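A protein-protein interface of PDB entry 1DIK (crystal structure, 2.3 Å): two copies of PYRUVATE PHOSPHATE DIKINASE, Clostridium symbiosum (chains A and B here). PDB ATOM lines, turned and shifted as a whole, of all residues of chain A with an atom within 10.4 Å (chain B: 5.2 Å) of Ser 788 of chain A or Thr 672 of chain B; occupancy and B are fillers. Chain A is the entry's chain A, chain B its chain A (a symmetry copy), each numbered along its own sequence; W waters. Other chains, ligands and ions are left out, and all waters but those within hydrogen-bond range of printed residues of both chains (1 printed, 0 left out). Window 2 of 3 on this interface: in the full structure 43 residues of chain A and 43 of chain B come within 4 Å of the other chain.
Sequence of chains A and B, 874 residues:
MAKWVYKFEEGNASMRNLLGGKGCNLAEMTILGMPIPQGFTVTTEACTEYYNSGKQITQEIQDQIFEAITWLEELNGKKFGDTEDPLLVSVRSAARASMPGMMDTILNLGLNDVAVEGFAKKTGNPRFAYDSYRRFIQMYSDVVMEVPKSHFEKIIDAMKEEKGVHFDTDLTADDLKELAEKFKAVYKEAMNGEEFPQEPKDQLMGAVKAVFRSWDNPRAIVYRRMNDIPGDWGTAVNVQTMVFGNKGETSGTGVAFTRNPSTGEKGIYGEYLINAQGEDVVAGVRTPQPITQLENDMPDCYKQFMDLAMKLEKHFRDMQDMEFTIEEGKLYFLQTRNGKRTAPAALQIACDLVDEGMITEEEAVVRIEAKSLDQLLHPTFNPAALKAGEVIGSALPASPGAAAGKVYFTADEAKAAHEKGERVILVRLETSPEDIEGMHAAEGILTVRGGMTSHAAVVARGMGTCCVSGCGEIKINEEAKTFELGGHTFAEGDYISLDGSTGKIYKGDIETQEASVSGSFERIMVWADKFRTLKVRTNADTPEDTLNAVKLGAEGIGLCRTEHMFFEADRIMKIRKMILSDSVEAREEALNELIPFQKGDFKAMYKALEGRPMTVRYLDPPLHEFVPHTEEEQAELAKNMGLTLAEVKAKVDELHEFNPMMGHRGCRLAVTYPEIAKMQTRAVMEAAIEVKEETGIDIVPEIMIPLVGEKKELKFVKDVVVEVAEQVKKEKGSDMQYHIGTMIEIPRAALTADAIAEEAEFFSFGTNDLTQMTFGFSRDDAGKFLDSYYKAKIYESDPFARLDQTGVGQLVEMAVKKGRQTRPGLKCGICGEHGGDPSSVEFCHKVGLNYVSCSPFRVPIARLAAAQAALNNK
Water W1 bridges ND1 of His 664 of chain B and NZ of Lys 784 of chain A.
Of the printed residues of chain B, Ser 788 of chain A touches Thr 672.
Printed residues of chain A within 4 Å of Thr 672 of chain B: Phe 785 (3.9 Å) and Ser 788 (3.8 Å).
No residue of chain A comes within 4 Å of Ala 670 of chain B.
Tyr 673 of chain B touches none of the printed residues of chain A.
Printed residues of chain B within 4 Å of Tyr 789 of chain A: Arg 668 (3.4 Å) and Val 671 (3.6 Å).
Printed residues of chain B within 4 Å of Ile 794 of chain A: Val 671.
The nearest residue of chain A that does not touch Thr 672 of chain B is Lys 784 of chain A (4.4 Å).
The nearest printed residue of chain A that does not touch His 664 of chain B is Asp 781 of chain A (4.8 Å).
CD of Lys 784 of chain A touches CB of His 664 of chain B, at 3.6 Å.
Phe 785 of chain A touches His 664 of chain B (CD2 to CD2, 3.7 Å).
CD of Arg 668 of chain B touches CZ of Phe 785 of chain A, at 3.7 Å.
Phe 785 of chain A touches Thr 672 of chain B.
Thr 672 of chain B touches Ser 788 of chain A (CG2 to OG, 3.8 Å).
OH of Tyr 789 of chain A touches CG of Arg 668 of chain B, at 3.4 Å.
Val 671 of chain B touches Tyr 789 of chain A.
Ile 794 of chain A touches Val 671 of chain B.
No position is printed for both chains.
NE2 of His 664 of chain B lies within hydrogen-bond range of O of Arg 668 of chain B (3.3 Å).
The backbone carbonyl oxygen of Tyr 789 of chain A is in hydrogen-bond range of the backbone NH of Tyr 795 of chain A.
O of Tyr 789 of chain A is in hydrogen-bond range of N of Ile 794 of chain A (2.8 Å).
A ring nitrogen (NE2) of His 664 of chain B sits at hydrogen-bond distance from the side-chain hydroxyl (OG1) of Thr 672 of chain B (2.9 Å).
The side-chain hydroxyl (OG1) of Thr 672 of chain B is in hydrogen-bond range of the backbone carbonyl oxygen (O) of Leu 669 of chain B, at 3.3 Å.
Printed residues of chain B that touch a printed residue of chain A: His 664, Arg 668, Val 671 and Thr 672.
Of the 19 printed residues of chain A, 5 touch a printed residue of chain B.
Hydrophobic or aromatic side chains of chain A that line the printed part of chain B: Phe 785, Tyr 789 and Ile 794.
Among the printed residues, 8 pairs touch across the chains.
Among the printed residues, no Asp or Glu carboxylate lies within 4 Å of a Lys or Arg side-chain nitrogen of the other chain.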
ATOM      1  N   ILE A 221      18.216   0.741  17.953  1.00  0.00           N
ATOM      2  CA  ILE A 221      19.167  -0.284  17.677  1.00  0.00           C
ATOM      3  C   ILE A 221      20.427  -0.060  18.512  1.00  0.00           C
ATOM      4  O   ILE A 221      20.811  -0.942  19.261  1.00  0.00           O
ATOM      5  CB  ILE A 221      19.426  -0.374  16.167  1.00  0.00           C
ATOM      6  CG1 ILE A 221      18.173  -0.952  15.473  1.00  0.00           C
ATOM      7  CG2 ILE A 221      20.678  -1.227  15.905  1.00  0.00           C
ATOM      8  CD1 ILE A 221      18.147  -0.759  13.959  1.00  0.00           C
ATOM      9  N   VAL A 222      21.010   1.127  18.509  1.00  0.00           N
ATOM     10  CA  VAL A 222      22.202   1.263  19.320  1.00  0.00           C
ATOM     11  C   VAL A 222      21.953   0.996  20.786  1.00  0.00           C
ATOM     12  O   VAL A 222      22.788   0.387  21.422  1.00  0.00           O
ATOM     13  CB  VAL A 222      22.938   2.601  19.157  1.00  0.00           C
ATOM     14  CG1 VAL A 222      24.203   2.599  20.013  1.00  0.00           C
ATOM     15  CG2 VAL A 222      23.331   2.808  17.718  1.00  0.00           C
ATOM     16  N   ARG A 225      21.592  -2.827  21.436  1.00  0.00           N
ATOM     17  CA  ARG A 225      22.854  -3.523  21.448  1.00  0.00           C
ATOM     18  C   ARG A 225      23.530  -3.194  22.771  1.00  0.00           C
ATOM     19  O   ARG A 225      23.928  -4.109  23.498  1.00  0.00           O
ATOM     20  CB  ARG A 225      23.738  -3.115  20.275  1.00  0.00           C
ATOM     21  CG  ARG A 225      24.879  -4.091  20.030  1.00  0.00           C
ATOM     22  CD  ARG A 225      26.060  -3.340  19.551  1.00  0.00           C
ATOM     23  NE  ARG A 225      25.758  -2.588  18.339  1.00  0.00           N
ATOM     24  CZ  ARG A 225      25.757  -1.260  18.247  1.00  0.00           C
ATOM     25  NH1 ARG A 225      26.027  -0.532  19.308  1.00  0.00           N
ATOM     26  NH2 ARG A 225      25.583  -0.650  17.082  1.00  0.00           N
ATOM     27  N   ASP A 781      40.696  -5.162  11.842  1.00  0.00           N
ATOM     28  CA  ASP A 781      40.207  -4.673  10.581  1.00  0.00           C
ATOM     29  C   ASP A 781      38.699  -4.649  10.438  1.00  0.00           C
ATOM     30  O   ASP A 781      38.187  -4.053   9.507  1.00  0.00           O
ATOM     31  CB  ASP A 781      40.832  -5.513   9.472  1.00  0.00           C
ATOM     32  CG  ASP A 781      42.330  -5.494   9.511  1.00  0.00           C
ATOM     33  OD1 ASP A 781      42.949  -4.413   9.474  1.00  0.00           O
ATOM     34  OD2 ASP A 781      42.910  -6.574   9.596  1.00  0.00           O
ATOM     35  N   ALA A 782      38.013  -5.236  11.410  1.00  0.00           N
ATOM     36  CA  ALA A 782      36.578  -5.407  11.415  1.00  0.00           C
ATOM     37  C   ALA A 782      35.778  -4.194  11.699  1.00  0.00           C
ATOM     38  O   ALA A 782      34.626  -4.120  11.324  1.00  0.00           O
ATOM     39  CB  ALA A 782      36.178  -6.564  12.378  1.00  0.00           C
ATOM     40  N   GLY A 783      36.353  -3.239  12.390  1.00  0.00           N
ATOM     41  CA  GLY A 783      35.598  -2.032  12.667  1.00  0.00           C
ATOM     42  C   GLY A 783      35.160  -1.246  11.433  1.00  0.00           C
ATOM     43  O   GLY A 783      34.181  -0.484  11.520  1.00  0.00           O
ATOM     44  N   LYS A 784      35.871  -1.398  10.307  1.00  0.00           N
ATOM     45  CA  LYS A 784      35.527  -0.706   9.051  1.00  0.00           C
ATOM     46  C   LYS A 784      34.264  -1.207   8.332  1.00  0.00           C
ATOM     47  O   LYS A 784      33.903  -0.695   7.260  1.00  0.00           O
ATOM     48  CB  LYS A 784      36.721  -0.705   8.077  1.00  0.00           C
ATOM     49  CG  LYS A 784      37.093  -2.042   7.505  1.00  0.00           C
ATOM     50  CD  LYS A 784      38.480  -2.020   6.922  1.00  0.00           C
ATOM     51  CE  LYS A 784      38.764  -0.750   6.152  1.00  0.00           C
ATOM     52  NZ  LYS A 784      39.974  -0.861   5.245  1.00  0.00           N
ATOM     53  N   PHE A 785      33.620  -2.231   8.884  1.00  0.00           N
ATOM     54  CA  PHE A 785      32.395  -2.741   8.319  1.00  0.00           C
ATOM     55  C   PHE A 785      31.421  -3.193   9.406  1.00  0.00           C
ATOM     56  O   PHE A 785      30.232  -3.378   9.169  1.00  0.00           O
ATOM     57  CB  PHE A 785      32.683  -3.879   7.306  1.00  0.00           C
ATOM     58  CG  PHE A 785      33.414  -5.094   7.884  1.00  0.00           C
ATOM     59  CD1 PHE A 785      32.736  -6.041   8.664  1.00  0.00           C
ATOM     60  CD2 PHE A 785      34.751  -5.324   7.579  1.00  0.00           C
ATOM     61  CE1 PHE A 785      33.355  -7.182   9.129  1.00  0.00           C
ATOM     62  CE2 PHE A 785      35.397  -6.488   8.041  1.00  0.00           C
ATOM     63  CZ  PHE A 785      34.696  -7.414   8.817  1.00  0.00           C
ATOM     64  N   LEU A 786      31.907  -3.297  10.625  1.00  0.00           N
ATOM     65  CA  LEU A 786      31.089  -3.794  11.718  1.00  0.00           C
ATOM     66  C   LEU A 786      29.953  -2.905  12.138  1.00  0.00           C
ATOM     67  O   LEU A 786      28.933  -3.389  12.572  1.00  0.00           O
ATOM     68  CB  LEU A 786      31.977  -4.168  12.912  1.00  0.00           C
ATOM     69  CG  LEU A 786      31.790  -5.537  13.563  1.00  0.00           C
ATOM     70  CD1 LEU A 786      31.666  -6.657  12.595  1.00  0.00           C
ATOM     71  CD2 LEU A 786      32.939  -5.754  14.451  1.00  0.00           C
ATOM     72  N   ASP A 787      30.124  -1.596  12.019  1.00  0.00           N
ATOM     73  CA  ASP A 787      29.046  -0.693  12.403  1.00  0.00           C
ATOM     74  C   ASP A 787      27.844  -0.887  11.465  1.00  0.00           C
ATOM     75  O   ASP A 787      26.735  -1.145  11.941  1.00  0.00           O
ATOM     76  CB  ASP A 787      29.517   0.742  12.461  1.00  0.00           C
ATOM     77  CG  ASP A 787      28.690   1.564  13.428  1.00  0.00           C
ATOM     78  OD1 ASP A 787      28.267   1.030  14.490  1.00  0.00           O
ATOM     79  OD2 ASP A 787      28.426   2.745  13.118  1.00  0.00           O
ATOM     80  N   SER A 788      28.140  -0.975  10.161  1.00  0.00           N
ATOM     81  CA  SER A 788      27.187  -1.234   9.094  1.00  0.00           C
ATOM     82  C   SER A 788      26.458  -2.506   9.365  1.00  0.00           C
ATOM     83  O   SER A 788      25.334  -2.684   8.993  1.00  0.00           O
ATOM     84  CB  SER A 788      27.898  -1.400   7.775  1.00  0.00           C
ATOM     85  OG  SER A 788      28.679  -0.265   7.502  1.00  0.00           O
ATOM     86  N   TYR A 789      27.127  -3.449   9.960  1.00  0.00           N
ATOM     87  CA  TYR A 789      26.468  -4.671  10.278  1.00  0.00           C
ATOM     88  C   TYR A 789      25.471  -4.508  11.385  1.00  0.00           C
ATOM     89  O   TYR A 789      24.420  -5.126  11.355  1.00  0.00           O
ATOM     90  CB  TYR A 789      27.503  -5.685  10.642  1.00  0.00           C
ATOM     91  CG  TYR A 789      27.979  -6.422   9.430  1.00  0.00           C
ATOM     92  CD1 TYR A 789      28.577  -5.753   8.339  1.00  0.00           C
ATOM     93  CD2 TYR A 789      27.864  -7.791   9.390  1.00  0.00           C
ATOM     94  CE1 TYR A 789      29.037  -6.441   7.265  1.00  0.00           C
ATOM     95  CE2 TYR A 789      28.321  -8.497   8.325  1.00  0.00           C
ATOM     96  CZ  TYR A 789      28.919  -7.839   7.254  1.00  0.00           C
ATOM     97  OH  TYR A 789      29.397  -8.664   6.240  1.00  0.00           O
ATOM     98  N   TYR A 790      25.776  -3.677  12.362  1.00  0.00           N
ATOM     99  CA  TYR A 790      24.867  -3.480  13.466  1.00  0.00           C
ATOM    100  C   TYR A 790      23.747  -2.646  12.953  1.00  0.00           C
ATOM    101  O   TYR A 790      22.599  -2.953  13.154  1.00  0.00           O
ATOM    102  CB  TYR A 790      25.562  -2.763  14.577  1.00  0.00           C
ATOM    103  CG  TYR A 790      26.778  -3.508  15.065  1.00  0.00           C
ATOM    104  CD1 TYR A 790      26.734  -4.887  15.307  1.00  0.00           C
ATOM    105  CD2 TYR A 790      27.961  -2.823  15.348  1.00  0.00           C
ATOM    106  CE1 TYR A 790      27.850  -5.554  15.822  1.00  0.00           C
ATOM    107  CE2 TYR A 790      29.063  -3.481  15.876  1.00  0.00           C
ATOM    108  CZ  TYR A 790      29.021  -4.835  16.104  1.00  0.00           C
ATOM    109  OH  TYR A 790      30.163  -5.482  16.567  1.00  0.00           O
ATOM    110  N   LYS A 791      24.096  -1.629  12.198  1.00  0.00           N
ATOM    111  CA  LYS A 791      23.114  -0.742  11.584  1.00  0.00           C
ATOM    112  C   LYS A 791      22.129  -1.525  10.719  1.00  0.00           C
ATOM    113  O   LYS A 791      20.935  -1.190  10.646  1.00  0.00           O
ATOM    114  CB  LYS A 791      23.833   0.327  10.757  1.00  0.00           C
ATOM    115  CG  LYS A 791      24.546   1.357  11.640  1.00  0.00           C
ATOM    116  CD  LYS A 791      25.208   2.430  10.817  1.00  0.00           C
ATOM    117  CE  LYS A 791      25.440   3.685  11.629  1.00  0.00           C
ATOM    118  NZ  LYS A 791      25.781   4.826  10.703  1.00  0.00           N
ATOM    119  N   ALA A 792      22.627  -2.576  10.085  1.00  0.00           N
ATOM    120  CA  ALA A 792      21.780  -3.404   9.237  1.00  0.00           C
ATOM    121  C   ALA A 792      21.136  -4.559   9.976  1.00  0.00           C
ATOM    122  O   ALA A 792      20.439  -5.366   9.361  1.00  0.00           O
ATOM    123  CB  ALA A 792      22.544  -3.929   8.033  1.00  0.00           C
ATOM    124  N   LYS A 793      21.377  -4.656  11.283  1.00  0.00           N
ATOM    125  CA  LYS A 793      20.811  -5.725  12.112  1.00  0.00           C
ATOM    126  C   LYS A 793      21.317  -7.102  11.733  1.00  0.00           C
ATOM    127  O   LYS A 793      20.708  -8.136  12.073  1.00  0.00           O
ATOM    128  CB  LYS A 793      19.286  -5.656  12.101  1.00  0.00           C
ATOM    129  CG  LYS A 793      18.731  -4.480  12.881  1.00  0.00           C
ATOM    130  CD  LYS A 793      17.425  -4.043  12.313  1.00  0.00           C
ATOM    131  CE  LYS A 793      17.685  -3.099  11.147  1.00  0.00           C
ATOM    132  NZ  LYS A 793      16.729  -3.379  10.033  1.00  0.00           N
ATOM    133  N   ILE A 794      22.431  -7.107  11.008  1.00  0.00           N
ATOM    134  CA  ILE A 794      23.040  -8.365  10.602  1.00  0.00           C
ATOM    135  C   ILE A 794      23.568  -9.094  11.886  1.00  0.00           C
ATOM    136  O   ILE A 794      23.318 -10.308  12.106  1.00  0.00           O
ATOM    137  CB  ILE A 794      24.124  -8.138   9.529  1.00  0.00           C
ATOM    138  CG1 ILE A 794      23.466  -7.924   8.162  1.00  0.00           C
ATOM    139  CG2 ILE A 794      25.034  -9.314   9.482  1.00  0.00           C
ATOM    140  CD1 ILE A 794      24.249  -7.068   7.234  1.00  0.00           C
ATOM    141  N   TYR A 795      24.168  -8.288  12.769  1.00  0.00           N
ATOM    142  CA  TYR A 795      24.708  -8.684  14.060  1.00  0.00           C
ATOM    143  C   TYR A 795      24.017  -7.814  15.099  1.00  0.00           C
ATOM    144  O   TYR A 795      24.038  -6.596  14.980  1.00  0.00           O
ATOM    145  CB  TYR A 795      26.210  -8.367  14.155  1.00  0.00           C
ATOM    146  CG  TYR A 795      27.114  -9.314  13.416  1.00  0.00           C
ATOM    147  CD1 TYR A 795      26.674 -10.577  13.064  1.00  0.00           C
ATOM    148  CD2 TYR A 795      28.367  -8.905  12.986  1.00  0.00           C
ATOM    149  CE1 TYR A 795      27.444 -11.425  12.279  1.00  0.00           C
ATOM    150  CE2 TYR A 795      29.159  -9.745  12.192  1.00  0.00           C
ATOM    151  CZ  TYR A 795      28.677 -11.014  11.828  1.00  0.00           C
ATOM    152  OH  TYR A 795      29.384 -11.833  10.942  1.00  0.00           O
ATOM    153  N   GLU A 796      23.443  -8.436  16.123  1.00  0.00           N
ATOM    154  CA  GLU A 796      22.807  -7.687  17.188  1.00  0.00           C
ATOM    155  C   GLU A 796      23.827  -7.374  18.289  1.00  0.00           C
ATOM    156  O   GLU A 796      23.673  -6.420  19.025  1.00  0.00           O
ATOM    157  CB  GLU A 796      21.749  -8.524  17.843  1.00  0.00           C
ATOM    158  CG  GLU A 796      20.424  -8.664  17.194  1.00  0.00           C
ATOM    159  CD  GLU A 796      19.585  -9.684  17.967  1.00  0.00           C
ATOM    160  OE1 GLU A 796      20.126 -10.363  18.876  1.00  0.00           O
ATOM    161  OE2 GLU A 796      18.379  -9.811  17.678  1.00  0.00           O
ATOM    162  N   ARG B 587      30.339   6.384  -6.647  1.00  0.00           N
ATOM    163  CA  ARG B 587      30.852   5.016  -6.795  1.00  0.00           C
ATOM    164  C   ARG B 587      29.980   4.316  -7.815  1.00  0.00           C
ATOM    165  O   ARG B 587      30.476   3.598  -8.667  1.00  0.00           O
ATOM    166  CB  ARG B 587      30.741   4.199  -5.501  1.00  0.00           C
ATOM    167  CG  ARG B 587      31.278   4.862  -4.285  1.00  0.00           C
ATOM    168  CD  ARG B 587      30.842   4.080  -3.086  1.00  0.00           C
ATOM    169  NE  ARG B 587      30.754   4.957  -1.929  1.00  0.00           N
ATOM    170  CZ  ARG B 587      29.838   4.838  -0.977  1.00  0.00           C
ATOM    171  NH1 ARG B 587      28.924   3.877  -1.039  1.00  0.00           N
ATOM    172  NH2 ARG B 587      29.857   5.654   0.072  1.00  0.00           N
ATOM    173  N   HIS B 664      38.106  -6.379   5.302  1.00  0.00           N
ATOM    174  CA  HIS B 664      36.940  -5.880   4.589  1.00  0.00           C
ATOM    175  C   HIS B 664      36.944  -6.363   3.157  1.00  0.00           C
ATOM    176  O   HIS B 664      37.411  -5.647   2.283  1.00  0.00           O
ATOM    177  CB  HIS B 664      36.955  -4.353   4.621  1.00  0.00           C
ATOM    178  CG  HIS B 664      35.637  -3.745   4.249  1.00  0.00           C
ATOM    179  ND1 HIS B 664      35.465  -2.390   4.059  1.00  0.00           N
ATOM    180  CD2 HIS B 664      34.430  -4.313   4.028  1.00  0.00           C
ATOM    181  CE1 HIS B 664      34.211  -2.152   3.745  1.00  0.00           C
ATOM    182  NE2 HIS B 664      33.565  -3.303   3.719  1.00  0.00           N
ATOM    183  N   ARG B 668      31.406  -8.726   2.752  1.00  0.00           N
ATOM    184  CA  ARG B 668      31.539  -7.517   3.564  1.00  0.00           C
ATOM    185  C   ARG B 668      31.519  -6.205   2.802  1.00  0.00           C
ATOM    186  O   ARG B 668      30.966  -5.238   3.277  1.00  0.00           O
ATOM    187  CB  ARG B 668      32.804  -7.606   4.409  1.00  0.00           C
ATOM    188  CG  ARG B 668      32.675  -8.664   5.437  1.00  0.00           C
ATOM    189  CD  ARG B 668      34.026  -9.182   5.666  1.00  0.00           C
ATOM    190  NE  ARG B 668      33.969 -10.561   6.098  1.00  0.00           N
ATOM    191  CZ  ARG B 668      34.949 -11.132   6.787  1.00  0.00           C
ATOM    192  NH1 ARG B 668      36.034 -10.448   7.109  1.00  0.00           N
ATOM    193  NH2 ARG B 668      34.815 -12.341   7.231  1.00  0.00           N
ATOM    194  N   LEU B 669      32.206  -6.159   1.663  1.00  0.00           N
ATOM    195  CA  LEU B 669      32.260  -4.984   0.784  1.00  0.00           C
ATOM    196  C   LEU B 669      30.896  -4.668   0.161  1.00  0.00           C
ATOM    197  O   LEU B 669      30.630  -3.545  -0.187  1.00  0.00           O
ATOM    198  CB  LEU B 669      33.210  -5.259  -0.369  1.00  0.00           C
ATOM    199  CG  LEU B 669      34.681  -5.445  -0.097  1.00  0.00           C
ATOM    200  CD1 LEU B 669      35.392  -6.037  -1.342  1.00  0.00           C
ATOM    201  CD2 LEU B 669      35.233  -4.106   0.287  1.00  0.00           C
ATOM    202  N   ALA B 670      30.124  -5.705  -0.124  1.00  0.00           N
ATOM    203  CA  ALA B 670      28.796  -5.611  -0.720  1.00  0.00           C
ATOM    204  C   ALA B 670      27.753  -5.190   0.309  1.00  0.00           C
ATOM    205  O   ALA B 670      26.626  -4.849  -0.025  1.00  0.00           O
ATOM    206  CB  ALA B 670      28.411  -6.960  -1.359  1.00  0.00           C
ATOM    207  N   VAL B 671      28.126  -5.219   1.570  1.00  0.00           N
ATOM    208  CA  VAL B 671      27.198  -4.827   2.601  1.00  0.00           C
ATOM    209  C   VAL B 671      27.391  -3.346   2.823  1.00  0.00           C
ATOM    210  O   VAL B 671      26.447  -2.646   3.181  1.00  0.00           O
ATOM    211  CB  VAL B 671      27.402  -5.633   3.900  1.00  0.00           C
ATOM    212  CG1 VAL B 671      26.578  -5.047   5.019  1.00  0.00           C
ATOM    213  CG2 VAL B 671      27.031  -7.061   3.673  1.00  0.00           C
ATOM    214  N   THR B 672      28.632  -2.887   2.652  1.00  0.00           N
ATOM    215  CA  THR B 672      28.980  -1.466   2.789  1.00  0.00           C
ATOM    216  C   THR B 672      28.864  -0.812   1.389  1.00  0.00           C
ATOM    217  O   THR B 672      28.577   0.371   1.259  1.00  0.00           O
ATOM    218  CB  THR B 672      30.419  -1.244   3.376  1.00  0.00           C
ATOM    219  OG1 THR B 672      31.397  -1.790   2.481  1.00  0.00           O
ATOM    220  CG2 THR B 672      30.584  -1.927   4.706  1.00  0.00           C
ATOM    221  N   TYR B 673      29.049  -1.602   0.350  1.00  0.00           N
ATOM    222  CA  TYR B 673      28.944  -1.122  -0.999  1.00  0.00           C
ATOM    223  C   TYR B 673      28.127  -2.079  -1.807  1.00  0.00           C
ATOM    224  O   TYR B 673      28.667  -2.754  -2.714  1.00  0.00           O
ATOM    225  CB  TYR B 673      30.284  -1.038  -1.638  1.00  0.00           C
ATOM    226  CG  TYR B 673      31.256  -0.255  -0.840  1.00  0.00           C
ATOM    227  CD1 TYR B 673      31.024   1.076  -0.543  1.00  0.00           C
ATOM    228  CD2 TYR B 673      32.444  -0.837  -0.421  1.00  0.00           C
ATOM    229  CE1 TYR B 673      31.948   1.816   0.142  1.00  0.00           C
ATOM    230  CE2 TYR B 673      33.377  -0.109   0.261  1.00  0.00           C
ATOM    231  CZ  TYR B 673      33.130   1.219   0.551  1.00  0.00           C
ATOM    232  OH  TYR B 673      34.062   1.911   1.303  1.00  0.00           O
ATOM    233  N   PRO B 674      26.802  -2.133  -1.536  1.00  0.00           N
ATOM    234  CA  PRO B 674      25.913  -3.039  -2.276  1.00  0.00           C
ATOM    235  C   PRO B 674      25.944  -2.699  -3.764  1.00  0.00           C
ATOM    236  O   PRO B 674      25.564  -3.490  -4.557  1.00  0.00           O
ATOM    237  CB  PRO B 674      24.526  -2.753  -1.697  1.00  0.00           C
ATOM    238  CG  PRO B 674      24.743  -1.951  -0.538  1.00  0.00           C
ATOM    239  CD  PRO B 674      26.009  -1.187  -0.743  1.00  0.00           C
ATOM    240  N   GLU B 675      26.435  -1.525  -4.121  1.00  0.00           N
ATOM    241  CA  GLU B 675      26.518  -1.078  -5.506  1.00  0.00           C
ATOM    242  C   GLU B 675      27.401  -1.971  -6.330  1.00  0.00           C
ATOM    243  O   GLU B 675      27.216  -2.050  -7.545  1.00  0.00           O
ATOM    244  CB  GLU B 675      27.077   0.332  -5.555  1.00  0.00           C
ATOM    245  CG  GLU B 675      26.701   1.105  -4.331  1.00  0.00           C
ATOM    246  CD  GLU B 675      27.873   1.494  -3.473  1.00  0.00           C
ATOM    247  OE1 GLU B 675      28.855   2.044  -4.018  1.00  0.00           O
ATOM    248  OE2 GLU B 675      27.764   1.357  -2.237  1.00  0.00           O
HETATM  249  O   HOH W   1      37.570  -0.831   2.967  1.00  0.00           O
